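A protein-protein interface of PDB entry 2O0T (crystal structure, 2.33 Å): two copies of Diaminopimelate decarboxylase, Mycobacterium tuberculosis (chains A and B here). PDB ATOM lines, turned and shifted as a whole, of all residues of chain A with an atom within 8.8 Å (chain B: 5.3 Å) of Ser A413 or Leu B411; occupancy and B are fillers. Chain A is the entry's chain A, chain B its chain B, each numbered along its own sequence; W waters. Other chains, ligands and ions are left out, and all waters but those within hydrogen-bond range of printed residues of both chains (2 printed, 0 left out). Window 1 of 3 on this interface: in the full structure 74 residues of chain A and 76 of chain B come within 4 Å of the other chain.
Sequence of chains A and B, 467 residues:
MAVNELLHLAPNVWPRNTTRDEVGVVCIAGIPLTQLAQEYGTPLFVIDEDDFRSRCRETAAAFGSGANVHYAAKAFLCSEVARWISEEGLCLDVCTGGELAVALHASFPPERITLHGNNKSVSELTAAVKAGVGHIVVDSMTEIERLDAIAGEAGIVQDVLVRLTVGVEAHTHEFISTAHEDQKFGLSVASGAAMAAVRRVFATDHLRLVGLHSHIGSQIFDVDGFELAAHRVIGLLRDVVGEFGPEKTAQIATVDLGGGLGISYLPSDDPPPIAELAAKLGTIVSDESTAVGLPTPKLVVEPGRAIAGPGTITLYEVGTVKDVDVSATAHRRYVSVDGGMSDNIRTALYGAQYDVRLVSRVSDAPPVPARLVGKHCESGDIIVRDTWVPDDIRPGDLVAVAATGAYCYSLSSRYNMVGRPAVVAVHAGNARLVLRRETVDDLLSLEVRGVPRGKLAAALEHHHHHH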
ATOM      1  N   GLY A 340     -23.476 -17.476  21.066  1.00  0.00           N
ATOM      2  CA  GLY A 340     -23.794 -17.902  22.412  1.00  0.00           C
ATOM      3  C   GLY A 340     -24.520 -16.826  23.179  1.00  0.00           C
ATOM      4  O   GLY A 340     -25.371 -16.141  22.631  1.00  0.00           O
ATOM      5  N   MET A 341     -24.141 -16.678  24.438  1.00  0.00           N
ATOM      6  CA  MET A 341     -24.840 -15.800  25.359  1.00  0.00           C
ATOM      7  C   MET A 341     -24.691 -14.353  25.004  1.00  0.00           C
ATOM      8  O   MET A 341     -25.531 -13.558  25.417  1.00  0.00           O
ATOM      9  CB  MET A 341     -24.446 -16.087  26.818  1.00  0.00           C
ATOM     10  CG  MET A 341     -22.987 -15.881  27.168  1.00  0.00           C
ATOM     11  SD  MET A 341     -22.666 -16.483  28.866  1.00  0.00           S
ATOM     12  CE  MET A 341     -23.082 -15.071  29.926  1.00  0.00           C
ATOM     13  N   SER A 342     -23.657 -14.023  24.217  1.00  0.00           N
ATOM     14  CA  SER A 342     -23.519 -12.712  23.524  1.00  0.00           C
ATOM     15  C   SER A 342     -24.705 -12.292  22.638  1.00  0.00           C
ATOM     16  O   SER A 342     -25.136 -11.126  22.715  1.00  0.00           O
ATOM     17  CB  SER A 342     -22.210 -12.661  22.704  1.00  0.00           C
ATOM     18  OG  SER A 342     -22.132 -13.780  21.820  1.00  0.00           O
ATOM     19  N   ASP A 343     -25.248 -13.213  21.822  1.00  0.00           N
ATOM     20  CA  ASP A 343     -26.420 -12.912  20.932  1.00  0.00           C
ATOM     21  C   ASP A 343     -27.760 -13.480  21.462  1.00  0.00           C
ATOM     22  O   ASP A 343     -28.826 -13.095  21.015  1.00  0.00           O
ATOM     23  CB  ASP A 343     -26.167 -13.397  19.480  1.00  0.00           C
ATOM     24  CG  ASP A 343     -25.874 -14.891  19.406  1.00  0.00           C
ATOM     25  OD1 ASP A 343     -24.706 -15.286  19.513  1.00  0.00           O
ATOM     26  OD2 ASP A 343     -26.814 -15.694  19.273  1.00  0.00           O
ATOM     27  N   ASN A 344     -27.697 -14.399  22.436  1.00  0.00           N
ATOM     28  CA  ASN A 344     -28.924 -14.962  23.017  1.00  0.00           C
ATOM     29  C   ASN A 344     -28.658 -15.367  24.466  1.00  0.00           C
ATOM     30  O   ASN A 344     -28.237 -16.529  24.763  1.00  0.00           O
ATOM     31  CB  ASN A 344     -29.423 -16.148  22.185  1.00  0.00           C
ATOM     32  CG  ASN A 344     -30.738 -16.744  22.690  1.00  0.00           C
ATOM     33  OD1 ASN A 344     -31.381 -16.217  23.598  1.00  0.00           O
ATOM     34  ND2 ASN A 344     -31.129 -17.875  22.093  1.00  0.00           N
ATOM     35  N   ILE A 345     -28.842 -14.396  25.356  1.00  0.00           N
ATOM     36  CA  ILE A 345     -28.585 -14.618  26.758  1.00  0.00           C
ATOM     37  C   ILE A 345     -29.799 -15.160  27.536  1.00  0.00           C
ATOM     38  O   ILE A 345     -29.702 -15.392  28.728  1.00  0.00           O
ATOM     39  CB  ILE A 345     -28.043 -13.296  27.416  1.00  0.00           C
ATOM     40  CG1 ILE A 345     -27.218 -13.638  28.667  1.00  0.00           C
ATOM     41  CG2 ILE A 345     -29.196 -12.273  27.619  1.00  0.00           C
ATOM     42  CD1 ILE A 345     -26.619 -12.502  29.284  1.00  0.00           C
ATOM     43  N   ALA A 348     -29.745 -18.563  29.589  1.00  0.00           N
ATOM     44  CA  ALA A 348     -29.056 -18.368  30.863  1.00  0.00           C
ATOM     45  C   ALA A 348     -29.816 -17.393  31.757  1.00  0.00           C
ATOM     46  O   ALA A 348     -29.915 -17.606  32.956  1.00  0.00           O
ATOM     47  CB  ALA A 348     -27.614 -17.924  30.669  1.00  0.00           C
ATOM     48  N   HIS A 376     -18.281 -19.103  24.252  1.00  0.00           N
ATOM     49  CA  HIS A 376     -17.837 -18.326  25.417  1.00  0.00           C
ATOM     50  C   HIS A 376     -17.204 -19.185  26.498  1.00  0.00           C
ATOM     51  O   HIS A 376     -17.606 -20.329  26.692  1.00  0.00           O
ATOM     52  CB  HIS A 376     -19.012 -17.542  26.007  1.00  0.00           C
ATOM     53  CG  HIS A 376     -19.462 -16.430  25.118  1.00  0.00           C
ATOM     54  ND1 HIS A 376     -20.545 -16.545  24.270  1.00  0.00           N
ATOM     55  CD2 HIS A 376     -18.912 -15.218  24.862  1.00  0.00           C
ATOM     56  CE1 HIS A 376     -20.691 -15.423  23.584  1.00  0.00           C
ATOM     57  NE2 HIS A 376     -19.689 -14.617  23.895  1.00  0.00           N
ATOM     58  N   GLU A 378     -17.337 -19.906  29.508  1.00  0.00           N
ATOM     59  CA  GLU A 378     -18.175 -20.029  30.679  1.00  0.00           C
ATOM     60  C   GLU A 378     -19.057 -21.269  30.481  1.00  0.00           C
ATOM     61  O   GLU A 378     -19.722 -21.397  29.444  1.00  0.00           O
ATOM     62  CB  GLU A 378     -19.053 -18.773  30.703  1.00  0.00           C
ATOM     63  CG  GLU A 378     -20.056 -18.751  31.788  1.00  0.00           C
ATOM     64  CD  GLU A 378     -20.607 -17.345  32.056  1.00  0.00           C
ATOM     65  OE1 GLU A 378     -19.916 -16.350  31.755  1.00  0.00           O
ATOM     66  OE2 GLU A 378     -21.722 -17.265  32.586  1.00  0.00           O
ATOM     67  N   CYS A 408     -33.312 -10.686  21.994  1.00  0.00           N
ATOM     68  CA  CYS A 408     -32.001 -11.397  21.941  1.00  0.00           C
ATOM     69  C   CYS A 408     -30.910 -10.383  21.535  1.00  0.00           C
ATOM     70  O   CYS A 408     -29.996 -10.135  22.278  1.00  0.00           O
ATOM     71  CB  CYS A 408     -32.032 -12.639  21.045  1.00  0.00           C
ATOM     72  SG  CYS A 408     -33.176 -13.989  21.584  1.00  0.00           S
ATOM     73  N   TYR A 409     -31.076  -9.780  20.363  1.00  0.00           N
ATOM     74  CA  TYR A 409     -30.281  -8.645  19.956  1.00  0.00           C
ATOM     75  C   TYR A 409     -30.366  -7.446  20.956  1.00  0.00           C
ATOM     76  O   TYR A 409     -29.351  -6.859  21.298  1.00  0.00           O
ATOM     77  CB  TYR A 409     -30.671  -8.220  18.542  1.00  0.00           C
ATOM     78  CG  TYR A 409     -29.657  -7.279  17.919  1.00  0.00           C
ATOM     79  CD1 TYR A 409     -29.765  -5.879  18.092  1.00  0.00           C
ATOM     80  CD2 TYR A 409     -28.615  -7.775  17.123  1.00  0.00           C
ATOM     81  CE1 TYR A 409     -28.813  -5.001  17.546  1.00  0.00           C
ATOM     82  CE2 TYR A 409     -27.672  -6.919  16.566  1.00  0.00           C
ATOM     83  CZ  TYR A 409     -27.776  -5.528  16.768  1.00  0.00           C
ATOM     84  OH  TYR A 409     -26.850  -4.679  16.191  1.00  0.00           O
ATOM     85  N   SER A 410     -31.569  -7.083  21.399  1.00  0.00           N
ATOM     86  CA  SER A 410     -31.725  -6.010  22.428  1.00  0.00           C
ATOM     87  C   SER A 410     -30.789  -6.225  23.623  1.00  0.00           C
ATOM     88  O   SER A 410     -30.201  -5.292  24.161  1.00  0.00           O
ATOM     89  CB  SER A 410     -33.142  -6.048  22.965  1.00  0.00           C
ATOM     90  OG  SER A 410     -34.027  -5.709  21.936  1.00  0.00           O
ATOM     91  N   LEU A 411     -30.638  -7.501  24.018  1.00  0.00           N
ATOM     92  CA  LEU A 411     -29.734  -7.847  25.113  1.00  0.00           C
ATOM     93  C   LEU A 411     -28.303  -8.197  24.743  1.00  0.00           C
ATOM     94  O   LEU A 411     -27.555  -8.560  25.658  1.00  0.00           O
ATOM     95  CB  LEU A 411     -30.308  -8.988  25.962  1.00  0.00           C
ATOM     96  CG  LEU A 411     -31.525  -8.592  26.775  1.00  0.00           C
ATOM     97  CD1 LEU A 411     -32.347  -9.856  27.045  1.00  0.00           C
ATOM     98  CD2 LEU A 411     -31.181  -7.799  28.047  1.00  0.00           C
ATOM     99  N   SER A 412     -27.919  -8.094  23.470  1.00  0.00           N
ATOM    100  CA  SER A 412     -26.564  -8.518  23.050  1.00  0.00           C
ATOM    101  C   SER A 412     -25.443  -7.774  23.786  1.00  0.00           C
ATOM    102  O   SER A 412     -25.586  -6.627  24.094  1.00  0.00           O
ATOM    103  CB  SER A 412     -26.349  -8.484  21.522  1.00  0.00           C
ATOM    104  OG  SER A 412     -26.635  -7.185  21.031  1.00  0.00           O
ATOM    105  N   SER A 413     -24.335  -8.468  24.047  1.00  0.00           N
ATOM    106  CA  SER A 413     -23.130  -7.898  24.666  1.00  0.00           C
ATOM    107  C   SER A 413     -21.883  -8.261  23.828  1.00  0.00           C
ATOM    108  O   SER A 413     -21.950  -9.006  22.842  1.00  0.00           O
ATOM    109  CB  SER A 413     -22.977  -8.473  26.068  1.00  0.00           C
ATOM    110  OG  SER A 413     -22.768  -9.883  26.010  1.00  0.00           O
ATOM    111  N   ARG A 414     -20.746  -7.704  24.197  1.00  0.00           N
ATOM    112  CA  ARG A 414     -19.474  -8.065  23.567  1.00  0.00           C
ATOM    113  C   ARG A 414     -18.674  -8.970  24.500  1.00  0.00           C
ATOM    114  O   ARG A 414     -17.453  -8.873  24.572  1.00  0.00           O
ATOM    115  CB  ARG A 414     -18.666  -6.787  23.222  1.00  0.00           C
ATOM    116  CG  ARG A 414     -19.349  -5.880  22.223  1.00  0.00           C
ATOM    117  CD  ARG A 414     -18.658  -4.533  22.146  1.00  0.00           C
ATOM    118  NE  ARG A 414     -19.138  -3.751  21.001  1.00  0.00           N
ATOM    119  CZ  ARG A 414     -18.900  -2.466  20.871  1.00  0.00           C
ATOM    120  NH1 ARG A 414     -18.175  -1.891  21.843  1.00  0.00           N
ATOM    121  NH2 ARG A 414     -19.373  -1.766  19.796  1.00  0.00           N
ATOM    122  N   TYR A 415     -19.374  -9.810  25.251  1.00  0.00           N
ATOM    123  CA  TYR A 415     -18.711 -10.770  26.150  1.00  0.00           C
ATOM    124  C   TYR A 415     -17.697 -11.596  25.397  1.00  0.00           C
ATOM    125  O   TYR A 415     -17.980 -12.071  24.288  1.00  0.00           O
ATOM    126  CB  TYR A 415     -19.758 -11.645  26.798  1.00  0.00           C
ATOM    127  CG  TYR A 415     -19.256 -12.421  27.998  1.00  0.00           C
ATOM    128  CD1 TYR A 415     -19.620 -13.746  28.159  1.00  0.00           C
ATOM    129  CD2 TYR A 415     -18.391 -11.832  28.945  1.00  0.00           C
ATOM    130  CE1 TYR A 415     -19.148 -14.488  29.242  1.00  0.00           C
ATOM    131  CE2 TYR A 415     -17.912 -12.560  30.033  1.00  0.00           C
ATOM    132  CZ  TYR A 415     -18.310 -13.899  30.170  1.00  0.00           C
ATOM    133  OH  TYR A 415     -17.897 -14.661  31.220  1.00  0.00           O
ATOM    134  N   ASN A 416     -16.486 -11.686  25.950  1.00  0.00           N
ATOM    135  CA  ASN A 416     -15.301 -12.221  25.220  1.00  0.00           C
ATOM    136  C   ASN A 416     -14.895 -11.522  23.936  1.00  0.00           C
ATOM    137  O   ASN A 416     -14.260 -12.126  23.067  1.00  0.00           O
ATOM    138  CB  ASN A 416     -15.443 -13.710  24.981  1.00  0.00           C
ATOM    139  CG  ASN A 416     -15.473 -14.482  26.279  1.00  0.00           C
ATOM    140  OD1 ASN A 416     -14.610 -14.291  27.141  1.00  0.00           O
ATOM    141  ND2 ASN A 416     -16.479 -15.315  26.450  1.00  0.00           N
ATOM    142  N   MET A 417     -15.218 -10.235  23.823  1.00  0.00           N
ATOM    143  CA  MET A 417     -14.905  -9.504  22.589  1.00  0.00           C
ATOM    144  C   MET A 417     -15.565 -10.183  21.367  1.00  0.00           C
ATOM    145  O   MET A 417     -14.977 -10.271  20.266  1.00  0.00           O
ATOM    146  CB  MET A 417     -13.376  -9.347  22.393  1.00  0.00           C
ATOM    147  CG  MET A 417     -12.734  -8.565  23.562  1.00  0.00           C
ATOM    148  SD  MET A 417     -13.249  -6.832  23.514  1.00  0.00           S
ATOM    149  CE  MET A 417     -12.423  -6.238  25.027  1.00  0.00           C
ATOM    150  N   VAL A 418     -16.771 -10.681  21.574  1.00  0.00           N
ATOM    151  CA  VAL A 418     -17.504 -11.285  20.482  1.00  0.00           C
ATOM    152  C   VAL A 418     -18.451 -10.176  19.941  1.00  0.00           C
ATOM    153  O   VAL A 418     -19.363  -9.721  20.643  1.00  0.00           O
ATOM    154  CB  VAL A 418     -18.211 -12.601  20.919  1.00  0.00           C
ATOM    155  CG1 VAL A 418     -19.135 -13.102  19.860  1.00  0.00           C
ATOM    156  CG2 VAL A 418     -17.186 -13.699  21.257  1.00  0.00           C
ATOM    157  N   GLY A 419     -18.177  -9.682  18.733  1.00  0.00           N
ATOM    158  CA  GLY A 419     -18.989  -8.604  18.171  1.00  0.00           C
ATOM    159  C   GLY A 419     -20.434  -9.032  17.891  1.00  0.00           C
ATOM    160  O   GLY A 419     -20.727 -10.227  17.693  1.00  0.00           O
ATOM    161  N   ARG A 420     -21.344  -8.072  17.931  1.00  0.00           N
ATOM    162  CA  ARG A 420     -22.730  -8.291  17.506  1.00  0.00           C
ATOM    163  C   ARG A 420     -22.824  -8.901  16.080  1.00  0.00           C
ATOM    164  O   ARG A 420     -22.088  -8.489  15.158  1.00  0.00           O
ATOM    165  CB  ARG A 420     -23.526  -6.977  17.548  1.00  0.00           C
ATOM    166  CG  ARG A 420     -23.851  -6.457  18.929  1.00  0.00           C
ATOM    167  CD  ARG A 420     -24.542  -5.030  18.822  1.00  0.00           C
ATOM    168  NE  ARG A 420     -25.665  -4.867  19.754  1.00  0.00           N
ATOM    169  CZ  ARG A 420     -26.528  -3.829  19.762  1.00  0.00           C
ATOM    170  NH1 ARG A 420     -27.535  -3.824  20.638  1.00  0.00           N
ATOM    171  NH2 ARG A 420     -26.383  -2.779  18.920  1.00  0.00           N
ATOM    172  N   PRO A 421     -23.715  -9.900  15.915  1.00  0.00           N
ATOM    173  CA  PRO A 421     -24.014 -10.475  14.584  1.00  0.00           C
ATOM    174  C   PRO A 421     -24.700  -9.479  13.669  1.00  0.00           C
ATOM    175  O   PRO A 421     -25.336  -8.515  14.132  1.00  0.00           O
ATOM    176  CB  PRO A 421     -24.984 -11.637  14.910  1.00  0.00           C
ATOM    177  CG  PRO A 421     -24.699 -11.970  16.317  1.00  0.00           C
ATOM    178  CD  PRO A 421     -24.437 -10.624  16.979  1.00  0.00           C
ATOM    179  N   GLU A 438     -20.461  -6.280  13.962  1.00  0.00           N
ATOM    180  CA  GLU A 438     -19.352  -5.536  14.608  1.00  0.00           C
ATOM    181  C   GLU A 438     -18.000  -6.126  14.241  1.00  0.00           C
ATOM    182  O   GLU A 438     -17.836  -7.388  14.051  1.00  0.00           O
ATOM    183  CB  GLU A 438     -19.519  -5.508  16.141  1.00  0.00           C
ATOM    184  CG  GLU A 438     -20.596  -4.530  16.578  1.00  0.00           C
ATOM    185  CD  GLU A 438     -20.739  -4.346  18.091  1.00  0.00           C
ATOM    186  OE1 GLU A 438     -20.330  -5.233  18.853  1.00  0.00           O
ATOM    187  OE2 GLU A 438     -21.314  -3.303  18.509  1.00  0.00           O
ATOM    188  N   LEU A 443     -15.098  -2.946  18.517  1.00  0.00           N
ATOM    189  CA  LEU A 443     -14.571  -3.372  19.825  1.00  0.00           C
ATOM    190  C   LEU A 443     -13.625  -2.379  20.462  1.00  0.00           C
ATOM    191  O   LEU A 443     -13.649  -2.246  21.635  1.00  0.00           O
ATOM    192  CB  LEU A 443     -13.807  -4.721  19.674  1.00  0.00           C
ATOM    193  CG  LEU A 443     -14.487  -6.059  20.009  1.00  0.00           C
ATOM    194  CD1 LEU A 443     -16.047  -6.079  19.900  1.00  0.00           C
ATOM    195  CD2 LEU A 443     -13.796  -7.216  19.213  1.00  0.00           C
ATOM    196  N   SER B 342     -27.922  -3.374  32.249  1.00  0.00           N
ATOM    197  CA  SER B 342     -27.005  -3.059  31.133  1.00  0.00           C
ATOM    198  C   SER B 342     -25.530  -2.935  31.526  1.00  0.00           C
ATOM    199  O   SER B 342     -24.676  -3.256  30.694  1.00  0.00           O
ATOM    200  CB  SER B 342     -27.430  -1.805  30.348  1.00  0.00           C
ATOM    201  OG  SER B 342     -27.392  -0.688  31.211  1.00  0.00           O
ATOM    202  N   ILE B 345     -25.369  -6.996  35.032  1.00  0.00           N
ATOM    203  CA  ILE B 345     -26.360  -8.017  34.855  1.00  0.00           C
ATOM    204  C   ILE B 345     -26.241  -9.193  35.834  1.00  0.00           C
ATOM    205  O   ILE B 345     -27.114 -10.096  35.852  1.00  0.00           O
ATOM    206  CB  ILE B 345     -26.314  -8.584  33.416  1.00  0.00           C
ATOM    207  CG1 ILE B 345     -27.582  -9.456  33.196  1.00  0.00           C
ATOM    208  CG2 ILE B 345     -24.982  -9.385  33.203  1.00  0.00           C
ATOM    209  CD1 ILE B 345     -28.219  -9.347  31.841  1.00  0.00           C
ATOM    210  N   ARG B 346     -25.206  -9.143  36.677  1.00  0.00           N
ATOM    211  CA  ARG B 346     -24.829 -10.252  37.570  1.00  0.00           C
ATOM    212  C   ARG B 346     -25.853 -10.637  38.612  1.00  0.00           C
ATOM    213  O   ARG B 346     -25.958 -11.810  38.975  1.00  0.00           O
ATOM    214  CB  ARG B 346     -23.483  -9.964  38.260  1.00  0.00           C
ATOM    215  CG  ARG B 346     -22.269  -9.912  37.285  1.00  0.00           C
ATOM    216  CD  ARG B 346     -20.901 -10.107  37.989  1.00  0.00           C
ATOM    217  NE  ARG B 346     -20.736 -11.424  38.649  1.00  0.00           N
ATOM    218  CZ  ARG B 346     -20.790 -11.612  39.977  1.00  0.00           C
ATOM    219  NH1 ARG B 346     -20.992 -10.594  40.817  1.00  0.00           N
ATOM    220  NH2 ARG B 346     -20.631 -12.809  40.487  1.00  0.00           N
ATOM    221  N   LEU B 349     -28.422 -12.365  36.594  1.00  0.00           N
ATOM    222  CA  LEU B 349     -27.920 -13.510  35.840  1.00  0.00           C
ATOM    223  C   LEU B 349     -27.548 -14.672  36.757  1.00  0.00           C
ATOM    224  O   LEU B 349     -27.923 -15.822  36.484  1.00  0.00           O
ATOM    225  CB  LEU B 349     -26.736 -13.110  34.984  1.00  0.00           C
ATOM    226  CG  LEU B 349     -26.131 -14.138  33.992  1.00  0.00           C
ATOM    227  CD1 LEU B 349     -27.198 -14.815  33.138  1.00  0.00           C
ATOM    228  CD2 LEU B 349     -25.034 -13.472  33.121  1.00  0.00           C
ATOM    229  N   TYR B 350     -26.843 -14.356  37.843  1.00  0.00           N
ATOM    230  CA  TYR B 350     -26.292 -15.373  38.708  1.00  0.00           C
ATOM    231  C   TYR B 350     -26.784 -15.254  40.137  1.00  0.00           C
ATOM    232  O   TYR B 350     -26.317 -15.957  41.004  1.00  0.00           O
ATOM    233  CB  TYR B 350     -24.771 -15.297  38.752  1.00  0.00           C
ATOM    234  CG  TYR B 350     -24.045 -15.253  37.432  1.00  0.00           C
ATOM    235  CD1 TYR B 350     -23.434 -14.080  37.027  1.00  0.00           C
ATOM    236  CD2 TYR B 350     -23.925 -16.393  36.619  1.00  0.00           C
ATOM    237  CE1 TYR B 350     -22.768 -13.997  35.866  1.00  0.00           C
ATOM    238  CE2 TYR B 350     -23.209 -16.346  35.439  1.00  0.00           C
ATOM    239  CZ  TYR B 350     -22.632 -15.147  35.072  1.00  0.00           C
ATOM    240  OH  TYR B 350     -21.928 -15.015  33.911  1.00  0.00           O
ATOM    241  N   TYR B 407     -16.465  -8.991  35.224  1.00  0.00           N
ATOM    242  CA  TYR B 407     -17.698  -9.458  34.610  1.00  0.00           C
ATOM    243  C   TYR B 407     -18.882  -8.484  34.649  1.00  0.00           C
ATOM    244  O   TYR B 407     -20.038  -8.917  34.592  1.00  0.00           O
ATOM    245  CB  TYR B 407     -18.105 -10.839  35.158  1.00  0.00           C
ATOM    246  CG  TYR B 407     -16.962 -11.875  35.118  1.00  0.00           C
ATOM    247  CD1 TYR B 407     -16.579 -12.490  33.910  1.00  0.00           C
ATOM    248  CD2 TYR B 407     -16.290 -12.250  36.287  1.00  0.00           C
ATOM    249  CE1 TYR B 407     -15.575 -13.411  33.876  1.00  0.00           C
ATOM    250  CE2 TYR B 407     -15.238 -13.180  36.245  1.00  0.00           C
ATOM    251  CZ  TYR B 407     -14.878 -13.747  35.033  1.00  0.00           C
ATOM    252  OH  TYR B 407     -13.840 -14.682  34.945  1.00  0.00           O
ATOM    253  N   CYS B 408     -18.675  -7.188  34.789  1.00  0.00           N
ATOM    254  CA  CYS B 408     -19.836  -6.327  34.775  1.00  0.00           C
ATOM    255  C   CYS B 408     -19.813  -5.562  33.439  1.00  0.00           C
ATOM    256  O   CYS B 408     -20.737  -5.651  32.619  1.00  0.00           O
ATOM    257  CB  CYS B 408     -19.791  -5.392  35.965  1.00  0.00           C
ATOM    258  SG  CYS B 408     -20.089  -6.158  37.508  1.00  0.00           S
ATOM    259  N   TYR B 409     -18.730  -4.830  33.215  1.00  0.00           N
ATOM    260  CA  TYR B 409     -18.505  -4.182  31.924  1.00  0.00           C
ATOM    261  C   TYR B 409     -18.377  -5.237  30.802  1.00  0.00           C
ATOM    262  O   TYR B 409     -18.950  -5.062  29.722  1.00  0.00           O
ATOM    263  CB  TYR B 409     -17.241  -3.280  32.002  1.00  0.00           C
ATOM    264  CG  TYR B 409     -17.102  -2.392  30.818  1.00  0.00           C
ATOM    265  CD1 TYR B 409     -16.447  -2.846  29.662  1.00  0.00           C
ATOM    266  CD2 TYR B 409     -17.669  -1.099  30.830  1.00  0.00           C
ATOM    267  CE1 TYR B 409     -16.373  -2.031  28.516  1.00  0.00           C
ATOM    268  CE2 TYR B 409     -17.600  -0.307  29.750  1.00  0.00           C
ATOM    269  CZ  TYR B 409     -16.936  -0.762  28.577  1.00  0.00           C
ATOM    270  OH  TYR B 409     -16.842   0.083  27.503  1.00  0.00           O
ATOM    271  N   SER B 410     -17.630  -6.316  31.074  1.00  0.00           N
ATOM    272  CA  SER B 410     -17.466  -7.425  30.136  1.00  0.00           C
ATOM    273  C   SER B 410     -18.812  -7.846  29.521  1.00  0.00           C
ATOM    274  O   SER B 410     -18.902  -8.198  28.315  1.00  0.00           O
ATOM    275  CB  SER B 410     -16.923  -8.606  30.915  1.00  0.00           C
ATOM    276  OG  SER B 410     -15.599  -8.724  30.611  1.00  0.00           O
ATOM    277  N   LEU B 411     -19.841  -7.798  30.360  1.00  0.00           N
ATOM    278  CA  LEU B 411     -21.139  -8.348  30.022  1.00  0.00           C
ATOM    279  C   LEU B 411     -22.132  -7.252  29.683  1.00  0.00           C
ATOM    280  O   LEU B 411     -23.308  -7.568  29.451  1.00  0.00           O
ATOM    281  CB  LEU B 411     -21.693  -9.182  31.187  1.00  0.00           C
ATOM    282  CG  LEU B 411     -21.105 -10.582  31.362  1.00  0.00           C
ATOM    283  CD1 LEU B 411     -21.443 -11.083  32.822  1.00  0.00           C
ATOM    284  CD2 LEU B 411     -21.620 -11.605  30.283  1.00  0.00           C
ATOM    285  N   SER B 412     -21.669  -6.002  29.632  1.00  0.00           N
ATOM    286  CA  SER B 412     -22.565  -4.858  29.344  1.00  0.00           C
ATOM    287  C   SER B 412     -23.264  -4.991  28.016  1.00  0.00           C
ATOM    288  O   SER B 412     -22.716  -5.540  27.063  1.00  0.00           O
ATOM    289  CB  SER B 412     -21.840  -3.500  29.423  1.00  0.00           C
ATOM    290  OG  SER B 412     -20.801  -3.401  28.442  1.00  0.00           O
ATOM    291  N   SER B 413     -24.470  -4.447  27.961  1.00  0.00           N
ATOM    292  CA  SER B 413     -25.317  -4.514  26.771  1.00  0.00           C
ATOM    293  C   SER B 413     -25.862  -3.102  26.447  1.00  0.00           C
ATOM    294  O   SER B 413     -25.644  -2.162  27.200  1.00  0.00           O
ATOM    295  CB  SER B 413     -26.470  -5.516  27.012  1.00  0.00           C
ATOM    296  OG  SER B 413     -27.388  -4.902  27.874  1.00  0.00           O
HETATM  297  O   HOH W   1     -15.545 -10.640  28.237  1.00  0.00           O
HETATM  298  O   HOH W   2     -20.210  -6.407  26.535  1.00  0.00           O
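Among the printed residues, pairs that only touch across the chains: Ser A413 with Ser B412, Ser A412 with Ser B413, Tyr A415 with Leu B411, Leu A411 with Ser B413, Ser A413 with Leu B411, Tyr A415 with Tyr B407, Met A341 with Leu B411, Arg A414 with Ser B410 and Ala A348 with Leu B349.
Water W1 bridges N of Asn A416 (2.7 Å) and OG of Ser B410 (3.1 Å). Water W2 lies within hydrogen-bond range of the backbone carbonyl oxygen of Ser B412 (2.7 Å), the backbone NH of Arg A414 (2.7 Å) and the backbone carbonyl oxygen of Ser B410 (2.8 Å).
The backbone carbonyl oxygen of Ser B410 sits close to the backbone NH of Tyr A415 (3.5 Å). OE2 of Glu A378 is in hydrogen-bond range of OH of Tyr B350 (2.6 Å).
Leu B411 touches just these residues of chain A: Met A341 (3.8 Å), Ser A413 (3.5 Å) and Tyr A415 (3.4 Å). Ser B410 touches just these residues of chain A: Arg A414 (3.9 Å) and Tyr A415 (3.4 Å). Of chain A, only Ser A413 (3.1 Å) comes within 4 Å of Ser B412. Of the printed residues of chain A, Tyr B407 touches Tyr A415 (3.7 Å). Of the printed residues of chain B, Tyr A415 touches Tyr B407, Ser B410 and Leu B411.
Of the 12 printed residues of chain B, 7 touch a printed residue of chain A. Hydrophobic or aromatic side chains of chain B within 4 Å of the printed part of chain A: Leu B349, Tyr B350, Tyr B407 and Leu B411. Hydrophobic or aromatic side chains of chain A that line the printed part of chain B: Met A341, Ala A348 and Tyr A415. Among the printed residues, 11 pairs touch across the chains. Among the printed residues, no Asp or Glu carboxylate lies within 4 Å of a Lys or Arg side-chain nitrogen of the other chain.
OG of Ser A413 lies close to N of Tyr A415 (3.5 Å). The backbone NH of Ser B413 is in hydrogen-bond range of the backbone carbonyl oxygen of Ser B342, at 3.0 Å. The backbone NH of Ser A413 lies within hydrogen-bond range of the backbone carbonyl oxygen of Ser A342 (3.1 Å). The side-chain carboxylate (OE1) of Glu A378 sits at hydrogen-bond distance from the side-chain hydroxyl (OH) of Tyr A415 (2.7 Å). O of Tyr A415 sits at hydrogen-bond distance from NE2 of His A376. NH2 of Arg A414 lies within salt-bridge range of OE2 of Glu A438 (2.8 Å).
Leu A411 touches Ser B413, and with the chains exchanged Ser A413 touches Leu B411. Ser A412 touches Ser B413, and with the chains exchanged Ser A413 touches Ser B412. Of the 11 pairs that touch across the chains among the printed residues, 4 have their exchanged pair printed and touching as well.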
